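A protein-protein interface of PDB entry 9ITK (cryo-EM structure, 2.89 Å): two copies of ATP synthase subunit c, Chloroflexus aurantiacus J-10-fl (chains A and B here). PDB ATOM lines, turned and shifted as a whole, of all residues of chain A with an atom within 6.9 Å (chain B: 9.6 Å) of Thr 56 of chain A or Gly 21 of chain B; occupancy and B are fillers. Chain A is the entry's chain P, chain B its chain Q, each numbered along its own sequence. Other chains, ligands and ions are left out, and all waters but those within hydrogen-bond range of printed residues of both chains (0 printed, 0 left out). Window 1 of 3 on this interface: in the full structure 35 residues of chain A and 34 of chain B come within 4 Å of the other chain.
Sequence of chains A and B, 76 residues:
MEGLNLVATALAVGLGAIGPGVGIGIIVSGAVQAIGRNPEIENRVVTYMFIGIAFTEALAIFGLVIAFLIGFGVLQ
The backbone carbonyl oxygen (O) of Gly 52 of chain A sits at hydrogen-bond distance from the side-chain hydroxyl (OG1) of Thr 56 of chain A (3.3 Å).
O of Ile 53 of chain A lies within hydrogen-bond range of OG1 of Thr 56 of chain A.
Gly 19 of chain A touches Gly 21 of chain B, but with the chains exchanged Gly 21 of chain A does not touch Gly 19 of chain B (9.3 Å).
Pro 20 of chain A touches Gly 21 of chain B, but with the chains exchanged Gly 21 of chain A does not touch Pro 20 of chain B (8.8 Å).
Thr 56 of chain A touches Gly 21 of chain B, but with the chains exchanged Gly 21 of chain A does not touch Thr 56 of chain B (13.5 Å).
Thr 56 of chain A touches Ile 24 of chain B, but with the chains exchanged Ile 24 of chain A does not touch Thr 56 of chain B (12.6 Å).
17 positions are printed for both chains.
N of Gly 16 of chain A sits at hydrogen-bond distance from O of Gly 14 of chain B (2.9 Å).
The backbone carbonyl oxygen (O) of Ile 26 of chain A sits at hydrogen-bond distance from the side-chain hydroxyl (OG) of Ser 29 of chain B.
Hydrophobic or aromatic side chains of chain A within 4 Å of the printed part of chain B: Ile 18, Pro 20, Val 22, Ile 26, Ile 27, Phe 55 and Leu 59.
Hydrophobic or aromatic side chains of chain B within 4 Å of the printed part of chain A: Ala 17, Ile 18, Val 22, Ile 24, Ile 26, Val 28, Ile 53 and Ala 60.
Thr 56 of chain A touches just these residues of chain B: Gly 21 and Ile 24.
Of chain B, only Ile 18 (3.3 Å), Gly 21 (3.5 Å) and Val 22 (3.3 Å) come within 4 Å of Gly 19 of chain A.
Printed residues of chain B within 4 Å of Pro 20 of chain A: Ala 17 (3.7 Å) and Gly 21 (3.8 Å).
Gly 23 of chain A touches just these residues of chain B: Gly 21 (3.3 Å) and Gly 25 (3.6 Å).
No residue of chain B comes within 4 Å of Ala 58 of chain A.
Of the printed residues of chain A, Val 22 of chain B touches Gly 19 and Val 22.
Printed residues of chain A within 4 Å of Ile 24 of chain B: Ile 27 (3.7 Å), Phe 55 (3.5 Å) and Thr 56 (3.5 Å).
Printed residues of chain A within 4 Å of Gly 14 of chain B: Gly 16 (2.9 Å).
Printed residues of chain A within 4 Å of Ala 17 of chain B: Gly 16 (3.8 Å), Pro 20 (3.7 Å) and Leu 59 (3.9 Å).
Thr 56 of chain B touches none of the printed residues of chain A.
Ile 51 of chain A touches none of the printed residues of chain B.
Among the printed residues, merely in contact across the chains: Gly 16 of chain A with Ala 17 of chain B, Gly 16 of chain A with Ile 18 of chain B, Ile 18 of chain A with Ile 18 of chain B, Gly 19 of chain A with Ile 18 of chain B, Gly 19 of chain A with Gly 21 of chain B, Gly 19 of chain A with Val 22 of chain B, Pro 20 of chain A with Ala 17 of chain B, Pro 20 of chain A with Gly 21 of chain B, Val 22 of chain A with Val 22 of chain B, Gly 23 of chain A with Gly 21 of chain B, Gly 23 of chain A with Gly 25 of chain B, Ile 26 of chain A with Gly 25 of chain B, Ile 26 of chain A with Ile 26 of chain B, Ile 27 of chain A with Ile 24 of chain B, Ile 27 of chain A with Gly 25 of chain B, Ile 27 of chain A with Val 28 of chain B, Gly 52 of chain A with Val 28 of chain B, Phe 55 of chain A with Ile 24 of chain B, Phe 55 of chain A with Ile 53 of chain B, Phe 55 of chain A with Glu 57 of chain B, Thr 56 of chain A with Gly 21 of chain B, Thr 56 of chain A with Ile 24 of chain B, Leu 59 of chain A with Ala 17 of chain B and Leu 59 of chain A with Ala 60 of chain B.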
ATOM      1  N   GLY A  16      -2.602   8.332 -15.637  1.00  0.00           N
ATOM      2  CA  GLY A  16      -1.515   7.386 -15.655  1.00  0.00           C
ATOM      3  C   GLY A  16      -1.037   6.973 -14.281  1.00  0.00           C
ATOM      4  O   GLY A  16      -0.367   5.943 -14.157  1.00  0.00           O
ATOM      5  N   ILE A  18      -3.483   6.713 -11.939  1.00  0.00           N
ATOM      6  CA  ILE A  18      -4.741   6.219 -11.395  1.00  0.00           C
ATOM      7  C   ILE A  18      -4.730   4.699 -11.433  1.00  0.00           C
ATOM      8  O   ILE A  18      -5.032   4.039 -10.433  1.00  0.00           O
ATOM      9  CB  ILE A  18      -5.943   6.780 -12.172  1.00  0.00           C
ATOM     10  CG1 ILE A  18      -5.932   8.306 -12.144  1.00  0.00           C
ATOM     11  CG2 ILE A  18      -7.239   6.243 -11.599  1.00  0.00           C
ATOM     12  CD1 ILE A  18      -6.814   8.931 -13.192  1.00  0.00           C
ATOM     13  N   GLY A  19      -4.386   4.137 -12.587  1.00  0.00           N
ATOM     14  CA  GLY A  19      -4.322   2.705 -12.749  1.00  0.00           C
ATOM     15  C   GLY A  19      -3.273   2.059 -11.869  1.00  0.00           C
ATOM     16  O   GLY A  19      -3.576   1.222 -11.016  1.00  0.00           O
ATOM     17  N   PRO A  20      -2.007   2.431 -12.070  1.00  0.00           N
ATOM     18  CA  PRO A  20      -0.949   1.892 -11.205  1.00  0.00           C
ATOM     19  C   PRO A  20      -1.171   2.168  -9.732  1.00  0.00           C
ATOM     20  O   PRO A  20      -0.787   1.346  -8.891  1.00  0.00           O
ATOM     21  CB  PRO A  20       0.307   2.590 -11.732  1.00  0.00           C
ATOM     22  CG  PRO A  20       0.010   2.824 -13.164  1.00  0.00           C
ATOM     23  CD  PRO A  20      -1.453   3.149 -13.230  1.00  0.00           C
ATOM     24  N   GLY A  21      -1.772   3.307  -9.387  1.00  0.00           N
ATOM     25  CA  GLY A  21      -2.076   3.564  -7.989  1.00  0.00           C
ATOM     26  C   GLY A  21      -3.000   2.513  -7.406  1.00  0.00           C
ATOM     27  O   GLY A  21      -2.746   1.973  -6.327  1.00  0.00           O
ATOM     28  N   VAL A  22      -4.080   2.198  -8.121  1.00  0.00           N
ATOM     29  CA  VAL A  22      -4.939   1.093  -7.712  1.00  0.00           C
ATOM     30  C   VAL A  22      -4.256  -0.238  -7.986  1.00  0.00           C
ATOM     31  O   VAL A  22      -4.445  -1.205  -7.239  1.00  0.00           O
ATOM     32  CB  VAL A  22      -6.300   1.180  -8.422  1.00  0.00           C
ATOM     33  CG1 VAL A  22      -7.230   0.099  -7.910  1.00  0.00           C
ATOM     34  CG2 VAL A  22      -6.914   2.546  -8.221  1.00  0.00           C
ATOM     35  N   GLY A  23      -3.458  -0.314  -9.052  1.00  0.00           N
ATOM     36  CA  GLY A  23      -2.837  -1.579  -9.411  1.00  0.00           C
ATOM     37  C   GLY A  23      -1.945  -2.124  -8.314  1.00  0.00           C
ATOM     38  O   GLY A  23      -2.009  -3.306  -7.978  1.00  0.00           O
ATOM     39  N   ILE A  24      -1.108  -1.262  -7.732  1.00  0.00           N
ATOM     40  CA  ILE A  24      -0.240  -1.702  -6.645  1.00  0.00           C
ATOM     41  C   ILE A  24      -1.066  -2.124  -5.442  1.00  0.00           C
ATOM     42  O   ILE A  24      -0.721  -3.088  -4.747  1.00  0.00           O
ATOM     43  CB  ILE A  24       0.761  -0.592  -6.273  1.00  0.00           C
ATOM     44  CG1 ILE A  24       1.668  -0.266  -7.453  1.00  0.00           C
ATOM     45  CG2 ILE A  24       1.602  -1.012  -5.085  1.00  0.00           C
ATOM     46  CD1 ILE A  24       2.221   1.135  -7.421  1.00  0.00           C
ATOM     47  N   GLY A  25      -2.169  -1.423  -5.178  1.00  0.00           N
ATOM     48  CA  GLY A  25      -3.012  -1.786  -4.053  1.00  0.00           C
ATOM     49  C   GLY A  25      -3.560  -3.193  -4.165  1.00  0.00           C
ATOM     50  O   GLY A  25      -3.617  -3.931  -3.181  1.00  0.00           O
ATOM     51  N   ILE A  26      -3.969  -3.584  -5.371  1.00  0.00           N
ATOM     52  CA  ILE A  26      -4.458  -4.939  -5.585  1.00  0.00           C
ATOM     53  C   ILE A  26      -3.317  -5.945  -5.484  1.00  0.00           C
ATOM     54  O   ILE A  26      -3.514  -7.069  -5.008  1.00  0.00           O
ATOM     55  CB  ILE A  26      -5.183  -5.015  -6.939  1.00  0.00           C
ATOM     56  CG1 ILE A  26      -6.318  -3.993  -6.975  1.00  0.00           C
ATOM     57  CG2 ILE A  26      -5.740  -6.397  -7.171  1.00  0.00           C
ATOM     58  CD1 ILE A  26      -7.095  -3.992  -8.260  1.00  0.00           C
ATOM     59  N   ILE A  27      -2.111  -5.561  -5.912  1.00  0.00           N
ATOM     60  CA  ILE A  27      -0.971  -6.480  -5.898  1.00  0.00           C
ATOM     61  C   ILE A  27      -0.648  -6.905  -4.473  1.00  0.00           C
ATOM     62  O   ILE A  27      -0.654  -8.095  -4.140  1.00  0.00           O
ATOM     63  CB  ILE A  27       0.255  -5.828  -6.558  1.00  0.00           C
ATOM     64  CG1 ILE A  27       0.019  -5.605  -8.045  1.00  0.00           C
ATOM     65  CG2 ILE A  27       1.476  -6.701  -6.353  1.00  0.00           C
ATOM     66  CD1 ILE A  27      -0.149  -6.859  -8.805  1.00  0.00           C
ATOM     67  N   ILE A  51       7.490  -8.296  -8.927  1.00  0.00           N
ATOM     68  CA  ILE A  51       7.355  -8.300 -10.381  1.00  0.00           C
ATOM     69  C   ILE A  51       6.105  -7.532 -10.792  1.00  0.00           C
ATOM     70  O   ILE A  51       6.131  -6.712 -11.717  1.00  0.00           O
ATOM     71  CB  ILE A  51       7.336  -9.741 -10.924  1.00  0.00           C
ATOM     72  CG1 ILE A  51       8.623 -10.475 -10.555  1.00  0.00           C
ATOM     73  CG2 ILE A  51       7.145  -9.746 -12.426  1.00  0.00           C
ATOM     74  CD1 ILE A  51       8.495 -11.977 -10.623  1.00  0.00           C
ATOM     75  N   GLY A  52       4.990  -7.789 -10.107  1.00  0.00           N
ATOM     76  CA  GLY A  52       3.762  -7.076 -10.419  1.00  0.00           C
ATOM     77  C   GLY A  52       3.827  -5.605 -10.056  1.00  0.00           C
ATOM     78  O   GLY A  52       3.332  -4.754 -10.799  1.00  0.00           O
ATOM     79  N   ILE A  53       4.435  -5.286  -8.912  1.00  0.00           N
ATOM     80  CA  ILE A  53       4.555  -3.890  -8.499  1.00  0.00           C
ATOM     81  C   ILE A  53       5.372  -3.107  -9.516  1.00  0.00           C
ATOM     82  O   ILE A  53       5.031  -1.973  -9.871  1.00  0.00           O
ATOM     83  CB  ILE A  53       5.168  -3.796  -7.090  1.00  0.00           C
ATOM     84  CG1 ILE A  53       4.146  -4.201  -6.031  1.00  0.00           C
ATOM     85  CG2 ILE A  53       5.679  -2.396  -6.817  1.00  0.00           C
ATOM     86  CD1 ILE A  53       4.677  -4.119  -4.622  1.00  0.00           C
ATOM     87  N   ALA A  54       6.461  -3.700 -10.000  1.00  0.00           N
ATOM     88  CA  ALA A  54       7.293  -3.022 -10.984  1.00  0.00           C
ATOM     89  C   ALA A  54       6.568  -2.860 -12.315  1.00  0.00           C
ATOM     90  O   ALA A  54       6.750  -1.851 -13.003  1.00  0.00           O
ATOM     91  CB  ALA A  54       8.596  -3.785 -11.167  1.00  0.00           C
ATOM     92  N   PHE A  55       5.754  -3.845 -12.701  1.00  0.00           N
ATOM     93  CA  PHE A  55       4.939  -3.703 -13.905  1.00  0.00           C
ATOM     94  C   PHE A  55       3.989  -2.518 -13.798  1.00  0.00           C
ATOM     95  O   PHE A  55       3.922  -1.677 -14.700  1.00  0.00           O
ATOM     96  CB  PHE A  55       4.147  -4.982 -14.163  1.00  0.00           C
ATOM     97  CG  PHE A  55       4.974  -6.121 -14.655  1.00  0.00           C
ATOM     98  CD1 PHE A  55       6.231  -5.906 -15.182  1.00  0.00           C
ATOM     99  CD2 PHE A  55       4.488  -7.412 -14.593  1.00  0.00           C
ATOM    100  CE1 PHE A  55       6.982  -6.960 -15.644  1.00  0.00           C
ATOM    101  CE2 PHE A  55       5.235  -8.465 -15.052  1.00  0.00           C
ATOM    102  CZ  PHE A  55       6.481  -8.239 -15.576  1.00  0.00           C
ATOM    103  N   THR A  56       3.230  -2.448 -12.704  1.00  0.00           N
ATOM    104  CA  THR A  56       2.309  -1.334 -12.518  1.00  0.00           C
ATOM    105  C   THR A  56       3.061  -0.016 -12.404  1.00  0.00           C
ATOM    106  O   THR A  56       2.689   0.978 -13.038  1.00  0.00           O
ATOM    107  CB  THR A  56       1.453  -1.567 -11.280  1.00  0.00           C
ATOM    108  OG1 THR A  56       2.303  -1.675 -10.134  1.00  0.00           O
ATOM    109  CG2 THR A  56       0.657  -2.847 -11.423  1.00  0.00           C
ATOM    110  N   GLU A  57       4.135   0.009 -11.610  1.00  0.00           N
ATOM    111  CA  GLU A  57       4.923   1.229 -11.477  1.00  0.00           C
ATOM    112  C   GLU A  57       5.545   1.641 -12.802  1.00  0.00           C
ATOM    113  O   GLU A  57       5.805   2.828 -13.018  1.00  0.00           O
ATOM    114  CB  GLU A  57       6.009   1.043 -10.419  1.00  0.00           C
ATOM    115  CG  GLU A  57       5.535   1.271  -8.996  1.00  0.00           C
ATOM    116  CD  GLU A  57       5.713   2.707  -8.546  1.00  0.00           C
ATOM    117  OE1 GLU A  57       5.674   3.612  -9.406  1.00  0.00           O
ATOM    118  OE2 GLU A  57       5.891   2.933  -7.331  1.00  0.00           O
ATOM    119  N   ALA A  58       5.784   0.682 -13.698  1.00  0.00           N
ATOM    120  CA  ALA A  58       6.375   1.008 -14.991  1.00  0.00           C
ATOM    121  C   ALA A  58       5.482   1.956 -15.778  1.00  0.00           C
ATOM    122  O   ALA A  58       5.961   2.923 -16.381  1.00  0.00           O
ATOM    123  CB  ALA A  58       6.628  -0.271 -15.789  1.00  0.00           C
ATOM    124  N   LEU A  59       4.175   1.694 -15.783  1.00  0.00           N
ATOM    125  CA  LEU A  59       3.261   2.546 -16.533  1.00  0.00           C
ATOM    126  C   LEU A  59       3.098   3.902 -15.866  1.00  0.00           C
ATOM    127  O   LEU A  59       2.938   4.921 -16.548  1.00  0.00           O
ATOM    128  CB  LEU A  59       1.913   1.853 -16.685  1.00  0.00           C
ATOM    129  CG  LEU A  59       2.027   0.623 -17.577  1.00  0.00           C
ATOM    130  CD1 LEU A  59       0.765  -0.222 -17.516  1.00  0.00           C
ATOM    131  CD2 LEU A  59       2.360   1.048 -18.991  1.00  0.00           C
ATOM    132  N   ALA A  60       3.128   3.934 -14.535  1.00  0.00           N
ATOM    133  CA  ALA A  60       3.036   5.205 -13.828  1.00  0.00           C
ATOM    134  C   ALA A  60       4.233   6.092 -14.135  1.00  0.00           C
ATOM    135  O   ALA A  60       4.084   7.304 -14.329  1.00  0.00           O
ATOM    136  CB  ALA A  60       2.926   4.958 -12.328  1.00  0.00           C
ATOM    137  N   ILE A  61       5.432   5.507 -14.175  1.00  0.00           N
ATOM    138  CA  ILE A  61       6.623   6.286 -14.492  1.00  0.00           C
ATOM    139  C   ILE A  61       6.594   6.758 -15.939  1.00  0.00           C
ATOM    140  O   ILE A  61       7.075   7.855 -16.248  1.00  0.00           O
ATOM    141  CB  ILE A  61       7.890   5.474 -14.181  1.00  0.00           C
ATOM    142  CG1 ILE A  61       7.915   5.085 -12.703  1.00  0.00           C
ATOM    143  CG2 ILE A  61       9.119   6.279 -14.503  1.00  0.00           C
ATOM    144  CD1 ILE A  61       7.933   6.267 -11.762  1.00  0.00           C
ATOM    145  N   VAL B  13      -0.531   8.759 -23.063  1.00  0.00           N
ATOM    146  CA  VAL B  13       0.114   7.949 -22.034  1.00  0.00           C
ATOM    147  C   VAL B  13      -0.694   7.942 -20.742  1.00  0.00           C
ATOM    148  O   VAL B  13      -0.797   6.908 -20.077  1.00  0.00           O
ATOM    149  CB  VAL B  13       1.555   8.443 -21.798  1.00  0.00           C
ATOM    150  CG1 VAL B  13       1.567   9.921 -21.451  1.00  0.00           C
ATOM    151  CG2 VAL B  13       2.225   7.628 -20.705  1.00  0.00           C
ATOM    152  N   GLY B  14      -1.275   9.081 -20.363  1.00  0.00           N
ATOM    153  CA  GLY B  14      -2.029   9.132 -19.121  1.00  0.00           C
ATOM    154  C   GLY B  14      -3.263   8.252 -19.149  1.00  0.00           C
ATOM    155  O   GLY B  14      -3.523   7.495 -18.210  1.00  0.00           O
ATOM    156  N   LEU B  15      -4.040   8.333 -20.230  1.00  0.00           N
ATOM    157  CA  LEU B  15      -5.244   7.518 -20.330  1.00  0.00           C
ATOM    158  C   LEU B  15      -4.919   6.073 -20.667  1.00  0.00           C
ATOM    159  O   LEU B  15      -5.651   5.164 -20.260  1.00  0.00           O
ATOM    160  CB  LEU B  15      -6.192   8.103 -21.375  1.00  0.00           C
ATOM    161  CG  LEU B  15      -6.999   9.324 -20.941  1.00  0.00           C
ATOM    162  CD1 LEU B  15      -7.688   9.955 -22.133  1.00  0.00           C
ATOM    163  CD2 LEU B  15      -8.013   8.935 -19.885  1.00  0.00           C
ATOM    164  N   GLY B  16      -3.834   5.835 -21.403  1.00  0.00           N
ATOM    165  CA  GLY B  16      -3.487   4.479 -21.782  1.00  0.00           C
ATOM    166  C   GLY B  16      -2.923   3.648 -20.652  1.00  0.00           C
ATOM    167  O   GLY B  16      -2.753   2.436 -20.814  1.00  0.00           O
ATOM    168  N   ALA B  17      -2.632   4.268 -19.511  1.00  0.00           N
ATOM    169  CA  ALA B  17      -2.042   3.553 -18.388  1.00  0.00           C
ATOM    170  C   ALA B  17      -3.044   3.224 -17.292  1.00  0.00           C
ATOM    171  O   ALA B  17      -2.825   2.275 -16.534  1.00  0.00           O
ATOM    172  CB  ALA B  17      -0.890   4.365 -17.793  1.00  0.00           C
ATOM    173  N   ILE B  18      -4.135   3.986 -17.181  1.00  0.00           N
ATOM    174  CA  ILE B  18      -5.076   3.751 -16.089  1.00  0.00           C
ATOM    175  C   ILE B  18      -5.836   2.448 -16.290  1.00  0.00           C
ATOM    176  O   ILE B  18      -6.227   1.795 -15.315  1.00  0.00           O
ATOM    177  CB  ILE B  18      -6.028   4.950 -15.930  1.00  0.00           C
ATOM    178  CG1 ILE B  18      -6.868   5.157 -17.186  1.00  0.00           C
ATOM    179  CG2 ILE B  18      -5.246   6.208 -15.630  1.00  0.00           C
ATOM    180  CD1 ILE B  18      -7.967   6.166 -16.993  1.00  0.00           C
ATOM    181  N   GLY B  19      -6.064   2.046 -17.534  1.00  0.00           N
ATOM    182  CA  GLY B  19      -6.752   0.808 -17.808  1.00  0.00           C
ATOM    183  C   GLY B  19      -5.916  -0.404 -17.446  1.00  0.00           C
ATOM    184  O   GLY B  19      -6.232  -1.149 -16.516  1.00  0.00           O
ATOM    185  N   PRO B  20      -4.829  -0.627 -18.190  1.00  0.00           N
ATOM    186  CA  PRO B  20      -3.927  -1.741 -17.865  1.00  0.00           C
ATOM    187  C   PRO B  20      -3.233  -1.603 -16.521  1.00  0.00           C
ATOM    188  O   PRO B  20      -2.716  -2.605 -16.013  1.00  0.00           O
ATOM    189  CB  PRO B  20      -2.910  -1.708 -19.008  1.00  0.00           C
ATOM    190  CG  PRO B  20      -3.636  -1.058 -20.129  1.00  0.00           C
ATOM    191  CD  PRO B  20      -4.530  -0.036 -19.505  1.00  0.00           C
ATOM    192  N   GLY B  21      -3.196  -0.405 -15.934  1.00  0.00           N
ATOM    193  CA  GLY B  21      -2.553  -0.249 -14.640  1.00  0.00           C
ATOM    194  C   GLY B  21      -3.199  -1.099 -13.564  1.00  0.00           C
ATOM    195  O   GLY B  21      -2.511  -1.655 -12.705  1.00  0.00           O
ATOM    196  N   VAL B  22      -4.525  -1.207 -13.590  1.00  0.00           N
ATOM    197  CA  VAL B  22      -5.208  -2.096 -12.661  1.00  0.00           C
ATOM    198  C   VAL B  22      -5.335  -3.502 -13.235  1.00  0.00           C
ATOM    199  O   VAL B  22      -5.506  -4.460 -12.478  1.00  0.00           O
ATOM    200  CB  VAL B  22      -6.590  -1.539 -12.281  1.00  0.00           C
ATOM    201  CG1 VAL B  22      -6.470  -0.119 -11.782  1.00  0.00           C
ATOM    202  CG2 VAL B  22      -7.535  -1.614 -13.453  1.00  0.00           C
ATOM    203  N   GLY B  23      -5.259  -3.647 -14.559  1.00  0.00           N
ATOM    204  CA  GLY B  23      -5.405  -4.965 -15.152  1.00  0.00           C
ATOM    205  C   GLY B  23      -4.311  -5.917 -14.718  1.00  0.00           C
ATOM    206  O   GLY B  23      -4.583  -7.017 -14.235  1.00  0.00           O
ATOM    207  N   ILE B  24      -3.053  -5.495 -14.859  1.00  0.00           N
ATOM    208  CA  ILE B  24      -1.950  -6.318 -14.380  1.00  0.00           C
ATOM    209  C   ILE B  24      -1.948  -6.370 -12.862  1.00  0.00           C
ATOM    210  O   ILE B  24      -1.404  -7.306 -12.266  1.00  0.00           O
ATOM    211  CB  ILE B  24      -0.611  -5.797 -14.932  1.00  0.00           C
ATOM    212  CG1 ILE B  24      -0.385  -4.352 -14.501  1.00  0.00           C
ATOM    213  CG2 ILE B  24      -0.584  -5.902 -16.446  1.00  0.00           C
ATOM    214  CD1 ILE B  24       0.909  -3.769 -14.994  1.00  0.00           C
ATOM    215  N   GLY B  25      -2.550  -5.375 -12.211  1.00  0.00           N
ATOM    216  CA  GLY B  25      -2.704  -5.440 -10.768  1.00  0.00           C
ATOM    217  C   GLY B  25      -3.590  -6.590 -10.335  1.00  0.00           C
ATOM    218  O   GLY B  25      -3.331  -7.240  -9.320  1.00  0.00           O
ATOM    219  N   ILE B  26      -4.655  -6.853 -11.095  1.00  0.00           N
ATOM    220  CA  ILE B  26      -5.522  -7.982 -10.787  1.00  0.00           C
ATOM    221  C   ILE B  26      -4.884  -9.287 -11.246  1.00  0.00           C
ATOM    222  O   ILE B  26      -5.170 -10.353 -10.688  1.00  0.00           O
ATOM    223  CB  ILE B  26      -6.909  -7.772 -11.421  1.00  0.00           C
ATOM    224  CG1 ILE B  26      -7.495  -6.431 -10.985  1.00  0.00           C
ATOM    225  CG2 ILE B  26      -7.859  -8.876 -11.019  1.00  0.00           C
ATOM    226  CD1 ILE B  26      -8.912  -6.206 -11.454  1.00  0.00           C
ATOM    227  N   ILE B  27      -4.011  -9.232 -12.255  1.00  0.00           N
ATOM    228  CA  ILE B  27      -3.373 -10.446 -12.766  1.00  0.00           C
ATOM    229  C   ILE B  27      -2.556 -11.116 -11.673  1.00  0.00           C
ATOM    230  O   ILE B  27      -2.808 -12.265 -11.295  1.00  0.00           O
ATOM    231  CB  ILE B  27      -2.489 -10.129 -13.983  1.00  0.00           C
ATOM    232  CG1 ILE B  27      -3.333  -9.687 -15.169  1.00  0.00           C
ATOM    233  CG2 ILE B  27      -1.684 -11.352 -14.363  1.00  0.00           C
ATOM    234  CD1 ILE B  27      -4.282 -10.729 -15.615  1.00  0.00           C
ATOM    235  N   VAL B  28      -1.556 -10.403 -11.156  1.00  0.00           N
ATOM    236  CA  VAL B  28      -0.667 -10.984 -10.156  1.00  0.00           C
ATOM    237  C   VAL B  28      -1.436 -11.310  -8.885  1.00  0.00           C
ATOM    238  O   VAL B  28      -1.236 -12.368  -8.278  1.00  0.00           O
ATOM    239  CB  VAL B  28       0.513 -10.038  -9.882  1.00  0.00           C
ATOM    240  CG1 VAL B  28       1.463 -10.651  -8.876  1.00  0.00           C
ATOM    241  CG2 VAL B  28       1.233  -9.707 -11.174  1.00  0.00           C
ATOM    242  N   SER B  29      -2.332 -10.416  -8.467  1.00  0.00           N
ATOM    243  CA  SER B  29      -3.121 -10.674  -7.267  1.00  0.00           C
ATOM    244  C   SER B  29      -3.976 -11.921  -7.427  1.00  0.00           C
ATOM    245  O   SER B  29      -4.093 -12.725  -6.496  1.00  0.00           O
ATOM    246  CB  SER B  29      -3.998  -9.470  -6.942  1.00  0.00           C
ATOM    247  OG  SER B  29      -4.816  -9.731  -5.817  1.00  0.00           O
ATOM    248  N   ILE B  53      -0.023 -10.680 -18.554  1.00  0.00           N
ATOM    249  CA  ILE B  53       0.572  -9.369 -18.309  1.00  0.00           C
ATOM    250  C   ILE B  53       1.081  -8.768 -19.611  1.00  0.00           C
ATOM    251  O   ILE B  53       0.821  -7.601 -19.923  1.00  0.00           O
ATOM    252  CB  ILE B  53       1.697  -9.476 -17.267  1.00  0.00           C
ATOM    253  CG1 ILE B  53       1.115  -9.725 -15.878  1.00  0.00           C
ATOM    254  CG2 ILE B  53       2.540  -8.222 -17.283  1.00  0.00           C
ATOM    255  CD1 ILE B  53       2.143 -10.109 -14.845  1.00  0.00           C
ATOM    256  N   THR B  56      -1.736  -7.821 -21.713  1.00  0.00           N
ATOM    257  CA  THR B  56      -2.351  -6.592 -21.221  1.00  0.00           C
ATOM    258  C   THR B  56      -1.458  -5.373 -21.422  1.00  0.00           C
ATOM    259  O   THR B  56      -1.927  -4.340 -21.914  1.00  0.00           O
ATOM    260  CB  THR B  56      -2.689  -6.718 -19.733  1.00  0.00           C
ATOM    261  OG1 THR B  56      -3.301  -7.987 -19.480  1.00  0.00           O
ATOM    262  CG2 THR B  56      -3.638  -5.612 -19.308  1.00  0.00           C
ATOM    263  N   GLU B  57      -0.179  -5.470 -21.050  1.00  0.00           N
ATOM    264  CA  GLU B  57       0.723  -4.330 -21.179  1.00  0.00           C
ATOM    265  C   GLU B  57       0.971  -3.951 -22.631  1.00  0.00           C
ATOM    266  O   GLU B  57       1.466  -2.850 -22.894  1.00  0.00           O
ATOM    267  CB  GLU B  57       2.051  -4.620 -20.479  1.00  0.00           C
ATOM    268  CG  GLU B  57       2.745  -3.378 -19.943  1.00  0.00           C
ATOM    269  CD  GLU B  57       3.611  -3.666 -18.732  1.00  0.00           C
ATOM    270  OE1 GLU B  57       3.494  -4.772 -18.167  1.00  0.00           O
ATOM    271  OE2 GLU B  57       4.401  -2.781 -18.342  1.00  0.00           O
ATOM    272  N   LEU B  59      -1.425  -3.317 -24.702  1.00  0.00           N
ATOM    273  CA  LEU B  59      -2.346  -2.198 -24.871  1.00  0.00           C
ATOM    274  C   LEU B  59      -1.799  -0.926 -24.247  1.00  0.00           C
ATOM    275  O   LEU B  59      -2.042   0.172 -24.759  1.00  0.00           O
ATOM    276  CB  LEU B  59      -3.696  -2.520 -24.239  1.00  0.00           C
ATOM    277  CG  LEU B  59      -4.582  -3.592 -24.862  1.00  0.00           C
ATOM    278  CD1 LEU B  59      -4.169  -4.974 -24.392  1.00  0.00           C
ATOM    279  CD2 LEU B  59      -6.015  -3.312 -24.490  1.00  0.00           C
ATOM    280  N   ALA B  60      -1.080  -1.055 -23.134  1.00  0.00           N
ATOM    281  CA  ALA B  60      -0.546   0.115 -22.449  1.00  0.00           C
ATOM    282  C   ALA B  60       0.568   0.765 -23.257  1.00  0.00           C
ATOM    283  O   ALA B  60       0.636   1.995 -23.361  1.00  0.00           O
ATOM    284  CB  ALA B  60      -0.054  -0.284 -21.061  1.00  0.00           C
ATOM    285  N   ILE B  61       1.458  -0.047 -23.831  1.00  0.00           N
ATOM    286  CA  ILE B  61       2.524   0.492 -24.666  1.00  0.00           C
ATOM    287  C   ILE B  61       1.964   1.158 -25.914  1.00  0.00           C
ATOM    288  O   ILE B  61       2.562   2.116 -26.420  1.00  0.00           O
ATOM    289  CB  ILE B  61       3.527  -0.619 -25.026  1.00  0.00           C
ATOM    290  CG1 ILE B  61       4.126  -1.219 -23.756  1.00  0.00           C
ATOM    291  CG2 ILE B  61       4.642  -0.082 -25.905  1.00  0.00           C
ATOM    292  CD1 ILE B  61       4.888  -0.220 -22.918  1.00  0.00           C
